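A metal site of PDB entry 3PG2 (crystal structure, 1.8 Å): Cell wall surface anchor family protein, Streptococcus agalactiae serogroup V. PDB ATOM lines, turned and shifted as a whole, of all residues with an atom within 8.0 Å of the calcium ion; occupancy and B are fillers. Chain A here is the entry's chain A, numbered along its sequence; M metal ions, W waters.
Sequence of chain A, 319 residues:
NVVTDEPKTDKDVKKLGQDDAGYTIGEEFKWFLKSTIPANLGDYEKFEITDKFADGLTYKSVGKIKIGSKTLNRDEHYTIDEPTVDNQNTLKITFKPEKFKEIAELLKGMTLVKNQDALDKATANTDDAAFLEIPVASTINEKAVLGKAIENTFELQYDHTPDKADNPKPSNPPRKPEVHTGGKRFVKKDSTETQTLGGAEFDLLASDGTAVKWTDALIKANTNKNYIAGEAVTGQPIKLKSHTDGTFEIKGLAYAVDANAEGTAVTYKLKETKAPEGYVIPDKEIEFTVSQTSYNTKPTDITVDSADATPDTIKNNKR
The side-chain carboxylate (OD2) of Asp 12 lies within salt-bridge range of the side-chain amino group (NZ) of Lys 34. OD2 of Asp 12 lies within hydrogen-bond range of N of Gly 17 (2.6 Å). O of Asp 12 lies within hydrogen-bond range of N of Phe 32, 2.9 Å away. The backbone carbonyl oxygen of Asp 10 sits at hydrogen-bond distance from the backbone NH of Lys 34 (2.8 Å).
Of the 23 residues printed, 4 come within 4 Å of the calcium ion. The nearest printed residue that does not touch the calcium ion is Lys 34 (4.5 Å).
The calcium ion is bound by OD1 of Asp 19 (2.3 Å), water W1 (2.4 Å), OD1 of Asp 12 (2.4 Å), O of Lys 11 (2.4 Å), water W2 (2.4 Å), OD2 of Asp 10 (2.5 Å) and OD1 of Asp 10 (2.6 Å). The calcium ion has seven donor atoms within binding distance.
Water W1 bridges OD2 of Asp 19 (2.7 Å) and O of Asp 120 (3.0 Å).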
ATOM      1  N   THR A   9      10.303  -6.351  20.418  1.00  0.00           N
ATOM      2  CA  THR A   9      11.661  -6.177  20.939  1.00  0.00           C
ATOM      3  C   THR A   9      12.551  -7.389  20.641  1.00  0.00           C
ATOM      4  O   THR A   9      12.081  -8.505  20.406  1.00  0.00           O
ATOM      5  CB  THR A   9      11.666  -5.933  22.479  1.00  0.00           C
ATOM      6  OG1 THR A   9      10.835  -6.911  23.119  1.00  0.00           O
ATOM      7  CG2 THR A   9      11.162  -4.524  22.813  1.00  0.00           C
ATOM      8  N   ASP A  10      13.849  -7.153  20.658  1.00  0.00           N
ATOM      9  CA  ASP A  10      14.830  -8.189  20.381  1.00  0.00           C
ATOM     10  C   ASP A  10      16.176  -7.762  20.954  1.00  0.00           C
ATOM     11  O   ASP A  10      16.407  -6.575  21.131  1.00  0.00           O
ATOM     12  CB  ASP A  10      14.979  -8.448  18.849  1.00  0.00           C
ATOM     13  CG  ASP A  10      16.041  -9.502  18.550  1.00  0.00           C
ATOM     14  OD1 ASP A  10      16.093 -10.505  19.286  1.00  0.00           O
ATOM     15  OD2 ASP A  10      16.851  -9.345  17.615  1.00  0.00           O
ATOM     16  N   LYS A  11      17.024  -8.725  21.281  1.00  0.00           N
ATOM     17  CA  LYS A  11      18.397  -8.425  21.725  1.00  0.00           C
ATOM     18  C   LYS A  11      19.406  -9.134  20.839  1.00  0.00           C
ATOM     19  O   LYS A  11      19.173 -10.300  20.440  1.00  0.00           O
ATOM     20  CB  LYS A  11      18.597  -8.861  23.190  1.00  0.00           C
ATOM     21  CG  LYS A  11      19.866  -8.287  23.847  1.00  0.00           C
ATOM     22  CD  LYS A  11      19.922  -8.703  25.325  1.00  0.00           C
ATOM     23  CE  LYS A  11      21.126  -8.101  26.016  1.00  0.00           C
ATOM     24  NZ  LYS A  11      21.147  -8.366  27.482  1.00  0.00           N
ATOM     25  N   ASP A  12      20.514  -8.457  20.518  1.00  0.00           N
ATOM     26  CA  ASP A  12      21.618  -9.074  19.732  1.00  0.00           C
ATOM     27  C   ASP A  12      22.900  -8.958  20.514  1.00  0.00           C
ATOM     28  O   ASP A  12      22.953  -8.261  21.540  1.00  0.00           O
ATOM     29  CB  ASP A  12      21.850  -8.376  18.365  1.00  0.00           C
ATOM     30  CG  ASP A  12      20.649  -8.506  17.382  1.00  0.00           C
ATOM     31  OD1 ASP A  12      19.756  -9.349  17.628  1.00  0.00           O
ATOM     32  OD2 ASP A  12      20.620  -7.735  16.379  1.00  0.00           O
ATOM     33  N   VAL A  13      23.966  -9.608  20.020  1.00  0.00           N
ATOM     34  CA  VAL A  13      25.313  -9.507  20.615  1.00  0.00           C
ATOM     35  C   VAL A  13      26.350  -9.389  19.490  1.00  0.00           C
ATOM     36  O   VAL A  13      26.140  -9.942  18.406  1.00  0.00           O
ATOM     37  CB  VAL A  13      25.655 -10.689  21.578  1.00  0.00           C
ATOM     38  CG1 VAL A  13      25.786 -12.051  20.850  1.00  0.00           C
ATOM     39  CG2 VAL A  13      26.918 -10.372  22.437  1.00  0.00           C
ATOM     40  N   LYS A  15      27.243  -7.713  16.967  1.00  0.00           N
ATOM     41  CA  LYS A  15      26.770  -6.799  15.915  1.00  0.00           C
ATOM     42  C   LYS A  15      25.302  -7.060  15.650  1.00  0.00           C
ATOM     43  O   LYS A  15      24.789  -8.128  15.999  1.00  0.00           O
ATOM     44  CB  LYS A  15      27.562  -7.028  14.619  1.00  0.00           C
ATOM     45  CG  LYS A  15      27.394  -8.435  14.009  1.00  0.00           C
ATOM     46  CD  LYS A  15      28.173  -8.531  12.708  1.00  0.00           C
ATOM     47  CE  LYS A  15      27.719  -9.732  11.883  1.00  0.00           C
ATOM     48  NZ  LYS A  15      28.581  -9.934  10.685  1.00  0.00           N
ATOM     49  N   LEU A  16      24.639  -6.111  14.975  1.00  0.00           N
ATOM     50  CA  LEU A  16      23.228  -6.293  14.627  1.00  0.00           C
ATOM     51  C   LEU A  16      22.991  -7.559  13.814  1.00  0.00           C
ATOM     52  O   LEU A  16      23.746  -7.858  12.881  1.00  0.00           O
ATOM     53  CB  LEU A  16      22.691  -5.029  13.899  1.00  0.00           C
ATOM     54  CG  LEU A  16      22.594  -3.774  14.774  1.00  0.00           C
ATOM     55  CD1 LEU A  16      22.244  -2.541  13.935  1.00  0.00           C
ATOM     56  CD2 LEU A  16      21.546  -3.944  15.886  1.00  0.00           C
ATOM     57  N   GLY A  17      21.974  -8.315  14.192  1.00  0.00           N
ATOM     58  CA  GLY A  17      21.634  -9.562  13.534  1.00  0.00           C
ATOM     59  C   GLY A  17      22.339 -10.802  14.087  1.00  0.00           C
ATOM     60  O   GLY A  17      21.985 -11.915  13.713  1.00  0.00           O
ATOM     61  N   GLN A  18      23.309 -10.615  14.987  1.00  0.00           N
ATOM     62  CA  GLN A  18      24.074 -11.747  15.529  1.00  0.00           C
ATOM     63  C   GLN A  18      23.528 -12.110  16.908  1.00  0.00           C
ATOM     64  O   GLN A  18      23.249 -11.220  17.702  1.00  0.00           O
ATOM     65  CB  GLN A  18      25.566 -11.412  15.631  1.00  0.00           C
ATOM     66  CG  GLN A  18      26.443 -12.615  16.124  1.00  0.00           C
ATOM     67  CD  GLN A  18      27.909 -12.569  15.693  1.00  0.00           C
ATOM     68  OE1 GLN A  18      28.758 -13.297  16.206  1.00  0.00           O
ATOM     69  NE2 GLN A  18      28.202 -11.712  14.745  1.00  0.00           N
ATOM     70  N   ASP A  19      23.374 -13.405  17.191  1.00  0.00           N
ATOM     71  CA  ASP A  19      22.754 -13.857  18.447  1.00  0.00           C
ATOM     72  C   ASP A  19      23.684 -14.699  19.347  1.00  0.00           C
ATOM     73  O   ASP A  19      23.322 -15.054  20.445  1.00  0.00           O
ATOM     74  CB  ASP A  19      21.451 -14.620  18.145  1.00  0.00           C
ATOM     75  CG  ASP A  19      20.324 -13.699  17.683  1.00  0.00           C
ATOM     76  OD1 ASP A  19      20.175 -12.575  18.228  1.00  0.00           O
ATOM     77  OD2 ASP A  19      19.610 -14.086  16.742  1.00  0.00           O
ATOM     78  N   ASP A  20      24.888 -14.978  18.864  1.00  0.00           N
ATOM     79  CA  ASP A  20      25.818 -15.871  19.565  1.00  0.00           C
ATOM     80  C   ASP A  20      27.255 -15.420  19.293  1.00  0.00           C
ATOM     81  O   ASP A  20      27.630 -15.235  18.138  1.00  0.00           O
ATOM     82  CB  ASP A  20      25.693 -17.326  19.045  1.00  0.00           C
ATOM     83  CG  ASP A  20      24.310 -17.927  19.313  1.00  0.00           C
ATOM     84  OD1 ASP A  20      24.048 -18.376  20.444  1.00  0.00           O
ATOM     85  OD2 ASP A  20      23.487 -17.922  18.363  1.00  0.00           O
ATOM     86  N   PHE A  32      23.048  -5.422  21.998  1.00  0.00           N
ATOM     87  CA  PHE A  32      22.185  -4.456  21.350  1.00  0.00           C
ATOM     88  C   PHE A  32      20.758  -4.687  21.781  1.00  0.00           C
ATOM     89  O   PHE A  32      20.207  -5.739  21.501  1.00  0.00           O
ATOM     90  CB  PHE A  32      22.281  -4.544  19.829  1.00  0.00           C
ATOM     91  CG  PHE A  32      23.649  -4.207  19.295  1.00  0.00           C
ATOM     92  CD1 PHE A  32      23.956  -2.900  18.909  1.00  0.00           C
ATOM     93  CD2 PHE A  32      24.638  -5.195  19.174  1.00  0.00           C
ATOM     94  CE1 PHE A  32      25.226  -2.591  18.419  1.00  0.00           C
ATOM     95  CE2 PHE A  32      25.909  -4.886  18.684  1.00  0.00           C
ATOM     96  CZ  PHE A  32      26.189  -3.590  18.316  1.00  0.00           C
ATOM     97  N   LYS A  34      16.993  -3.832  21.260  1.00  0.00           N
ATOM     98  CA  LYS A  34      16.324  -3.334  20.038  1.00  0.00           C
ATOM     99  C   LYS A  34      14.809  -3.278  20.228  1.00  0.00           C
ATOM    100  O   LYS A  34      14.228  -4.191  20.838  1.00  0.00           O
ATOM    101  CB  LYS A  34      16.627  -4.251  18.838  1.00  0.00           C
ATOM    102  CG  LYS A  34      18.112  -4.572  18.628  1.00  0.00           C
ATOM    103  CD  LYS A  34      18.308  -5.941  17.970  1.00  0.00           C
ATOM    104  CE  LYS A  34      17.865  -5.931  16.486  1.00  0.00           C
ATOM    105  NZ  LYS A  34      17.838  -7.362  16.006  1.00  0.00           N
ATOM    106  N   GLN A 116       8.227  -8.255  13.981  1.00  0.00           N
ATOM    107  CA  GLN A 116       9.241  -8.996  14.761  1.00  0.00           C
ATOM    108  C   GLN A 116      10.350  -9.643  13.919  1.00  0.00           C
ATOM    109  O   GLN A 116      11.531  -9.505  14.231  1.00  0.00           O
ATOM    110  CB  GLN A 116       8.543 -10.091  15.575  1.00  0.00           C
ATOM    111  CG  GLN A 116       9.486 -10.886  16.512  1.00  0.00           C
ATOM    112  CD  GLN A 116       9.804 -10.098  17.769  1.00  0.00           C
ATOM    113  OE1 GLN A 116       8.895  -9.760  18.522  1.00  0.00           O
ATOM    114  NE2 GLN A 116      11.076  -9.746  17.970  1.00  0.00           N
ATOM    115  N   LEU A 119      12.762  -7.159  12.557  1.00  0.00           N
ATOM    116  CA  LEU A 119      13.604  -6.633  13.657  1.00  0.00           C
ATOM    117  C   LEU A 119      14.720  -7.627  14.002  1.00  0.00           C
ATOM    118  O   LEU A 119      15.907  -7.257  14.091  1.00  0.00           O
ATOM    119  CB  LEU A 119      12.770  -6.328  14.898  1.00  0.00           C
ATOM    120  CG  LEU A 119      13.552  -5.721  16.068  1.00  0.00           C
ATOM    121  CD1 LEU A 119      14.105  -4.298  15.718  1.00  0.00           C
ATOM    122  CD2 LEU A 119      12.691  -5.665  17.320  1.00  0.00           C
ATOM    123  N   ASP A 120      14.327  -8.894  14.150  1.00  0.00           N
ATOM    124  CA  ASP A 120      15.233 -10.000  14.480  1.00  0.00           C
ATOM    125  C   ASP A 120      16.349 -10.143  13.469  1.00  0.00           C
ATOM    126  O   ASP A 120      17.486 -10.468  13.824  1.00  0.00           O
ATOM    127  CB  ASP A 120      14.486 -11.333  14.514  1.00  0.00           C
ATOM    128  CG  ASP A 120      13.575 -11.471  15.738  1.00  0.00           C
ATOM    129  OD1 ASP A 120      13.647 -10.648  16.666  1.00  0.00           O
ATOM    130  OD2 ASP A 120      12.748 -12.417  15.729  1.00  0.00           O
ATOM    131  N   LYS A 121      16.014  -9.930  12.206  1.00  0.00           N
ATOM    132  CA  LYS A 121      16.926 -10.186  11.100  1.00  0.00           C
ATOM    133  C   LYS A 121      17.760  -8.987  10.702  1.00  0.00           C
ATOM    134  O   LYS A 121      18.652  -9.108   9.864  1.00  0.00           O
ATOM    135  CB  LYS A 121      16.151 -10.719   9.877  1.00  0.00           C
ATOM    136  CG  LYS A 121      15.678 -12.148  10.053  1.00  0.00           C
ATOM    137  CD  LYS A 121      15.166 -12.725   8.732  1.00  0.00           C
ATOM    138  CE  LYS A 121      14.343 -13.999   8.879  1.00  0.00           C
ATOM    139  NZ  LYS A 121      14.338 -14.677  10.223  1.00  0.00           N
ATOM    140  N   ALA A 122      17.486  -7.809  11.293  1.00  0.00           N
ATOM    141  CA  ALA A 122      18.126  -6.574  10.849  1.00  0.00           C
ATOM    142  C   ALA A 122      19.626  -6.622  11.124  1.00  0.00           C
ATOM    143  O   ALA A 122      20.063  -6.954  12.242  1.00  0.00           O
ATOM    144  CB  ALA A 122      17.471  -5.348  11.511  1.00  0.00           C
ATOM    145  N   PRO A 173      11.905  -9.841  24.011  1.00  0.00           N
ATOM    146  CA  PRO A 173      12.518 -10.614  22.929  1.00  0.00           C
ATOM    147  C   PRO A 173      12.039 -12.054  22.952  1.00  0.00           C
ATOM    148  O   PRO A 173      12.106 -12.692  24.003  1.00  0.00           O
ATOM    149  CB  PRO A 173      14.026 -10.551  23.250  1.00  0.00           C
ATOM    150  CG  PRO A 173      14.183  -9.200  23.930  1.00  0.00           C
ATOM    151  CD  PRO A 173      12.925  -9.096  24.786  1.00  0.00           C
ATOM    152  N   PRO A 174      11.506 -12.555  21.829  1.00  0.00           N
ATOM    153  CA  PRO A 174      11.078 -13.965  21.844  1.00  0.00           C
ATOM    154  C   PRO A 174      12.261 -14.933  22.018  1.00  0.00           C
ATOM    155  O   PRO A 174      12.102 -16.013  22.595  1.00  0.00           O
ATOM    156  CB  PRO A 174      10.475 -14.177  20.464  1.00  0.00           C
ATOM    157  CG  PRO A 174      10.177 -12.821  19.928  1.00  0.00           C
ATOM    158  CD  PRO A 174      11.115 -11.848  20.600  1.00  0.00           C
ATOM    159  N   ARG A 175      13.434 -14.539  21.506  1.00  0.00           N
ATOM    160  CA  ARG A 175      14.651 -15.361  21.538  1.00  0.00           C
ATOM    161  C   ARG A 175      15.786 -14.533  22.119  1.00  0.00           C
ATOM    162  O   ARG A 175      15.865 -13.329  21.857  1.00  0.00           O
ATOM    163  CB  ARG A 175      14.976 -15.776  20.105  1.00  0.00           C
ATOM    164  CG  ARG A 175      13.990 -16.763  19.474  1.00  0.00           C
ATOM    165  CD  ARG A 175      13.998 -16.684  17.942  1.00  0.00           C
ATOM    166  NE  ARG A 175      13.186 -15.566  17.440  1.00  0.00           N
ATOM    167  CZ  ARG A 175      11.856 -15.544  17.370  1.00  0.00           C
ATOM    168  NH1 ARG A 175      11.126 -16.579  17.756  1.00  0.00           N
ATOM    169  NH2 ARG A 175      11.237 -14.466  16.901  1.00  0.00           N
ATOM    170  N   LYS A 176      16.667 -15.164  22.891  1.00  0.00           N
ATOM    171  CA  LYS A 176      17.741 -14.490  23.646  1.00  0.00           C
ATOM    172  C   LYS A 176      19.130 -14.765  23.063  1.00  0.00           C
ATOM    173  O   LYS A 176      19.438 -15.937  22.745  1.00  0.00           O
ATOM    174  CB  LYS A 176      17.758 -14.985  25.095  1.00  0.00           C
ATOM    175  CG  LYS A 176      16.472 -14.745  25.915  1.00  0.00           C
ATOM    176  CD  LYS A 176      16.661 -15.364  27.282  1.00  0.00           C
ATOM    177  CE  LYS A 176      15.347 -15.423  28.070  1.00  0.00           C
ATOM    178  NZ  LYS A 176      15.583 -15.826  29.495  1.00  0.00           N
ATOM    179  N   PRO A 177      19.979 -13.736  22.934  1.00  0.00           N
ATOM    180  CA  PRO A 177      21.376 -13.938  22.528  1.00  0.00           C
ATOM    181  C   PRO A 177      22.227 -14.431  23.708  1.00  0.00           C
ATOM    182  O   PRO A 177      21.795 -14.339  24.863  1.00  0.00           O
ATOM    183  CB  PRO A 177      21.817 -12.540  22.095  1.00  0.00           C
ATOM    184  CG  PRO A 177      21.001 -11.611  22.989  1.00  0.00           C
ATOM    185  CD  PRO A 177      19.658 -12.306  23.125  1.00  0.00           C
HETATM  186 CA    CA M   1      18.395 -11.177  18.340  1.00  0.00          CA
HETATM  187  O   HOH W   1      17.837 -12.134  16.248  1.00  0.00           O
HETATM  188  O   HOH W   2      17.590 -13.110  19.611  1.00  0.00           O
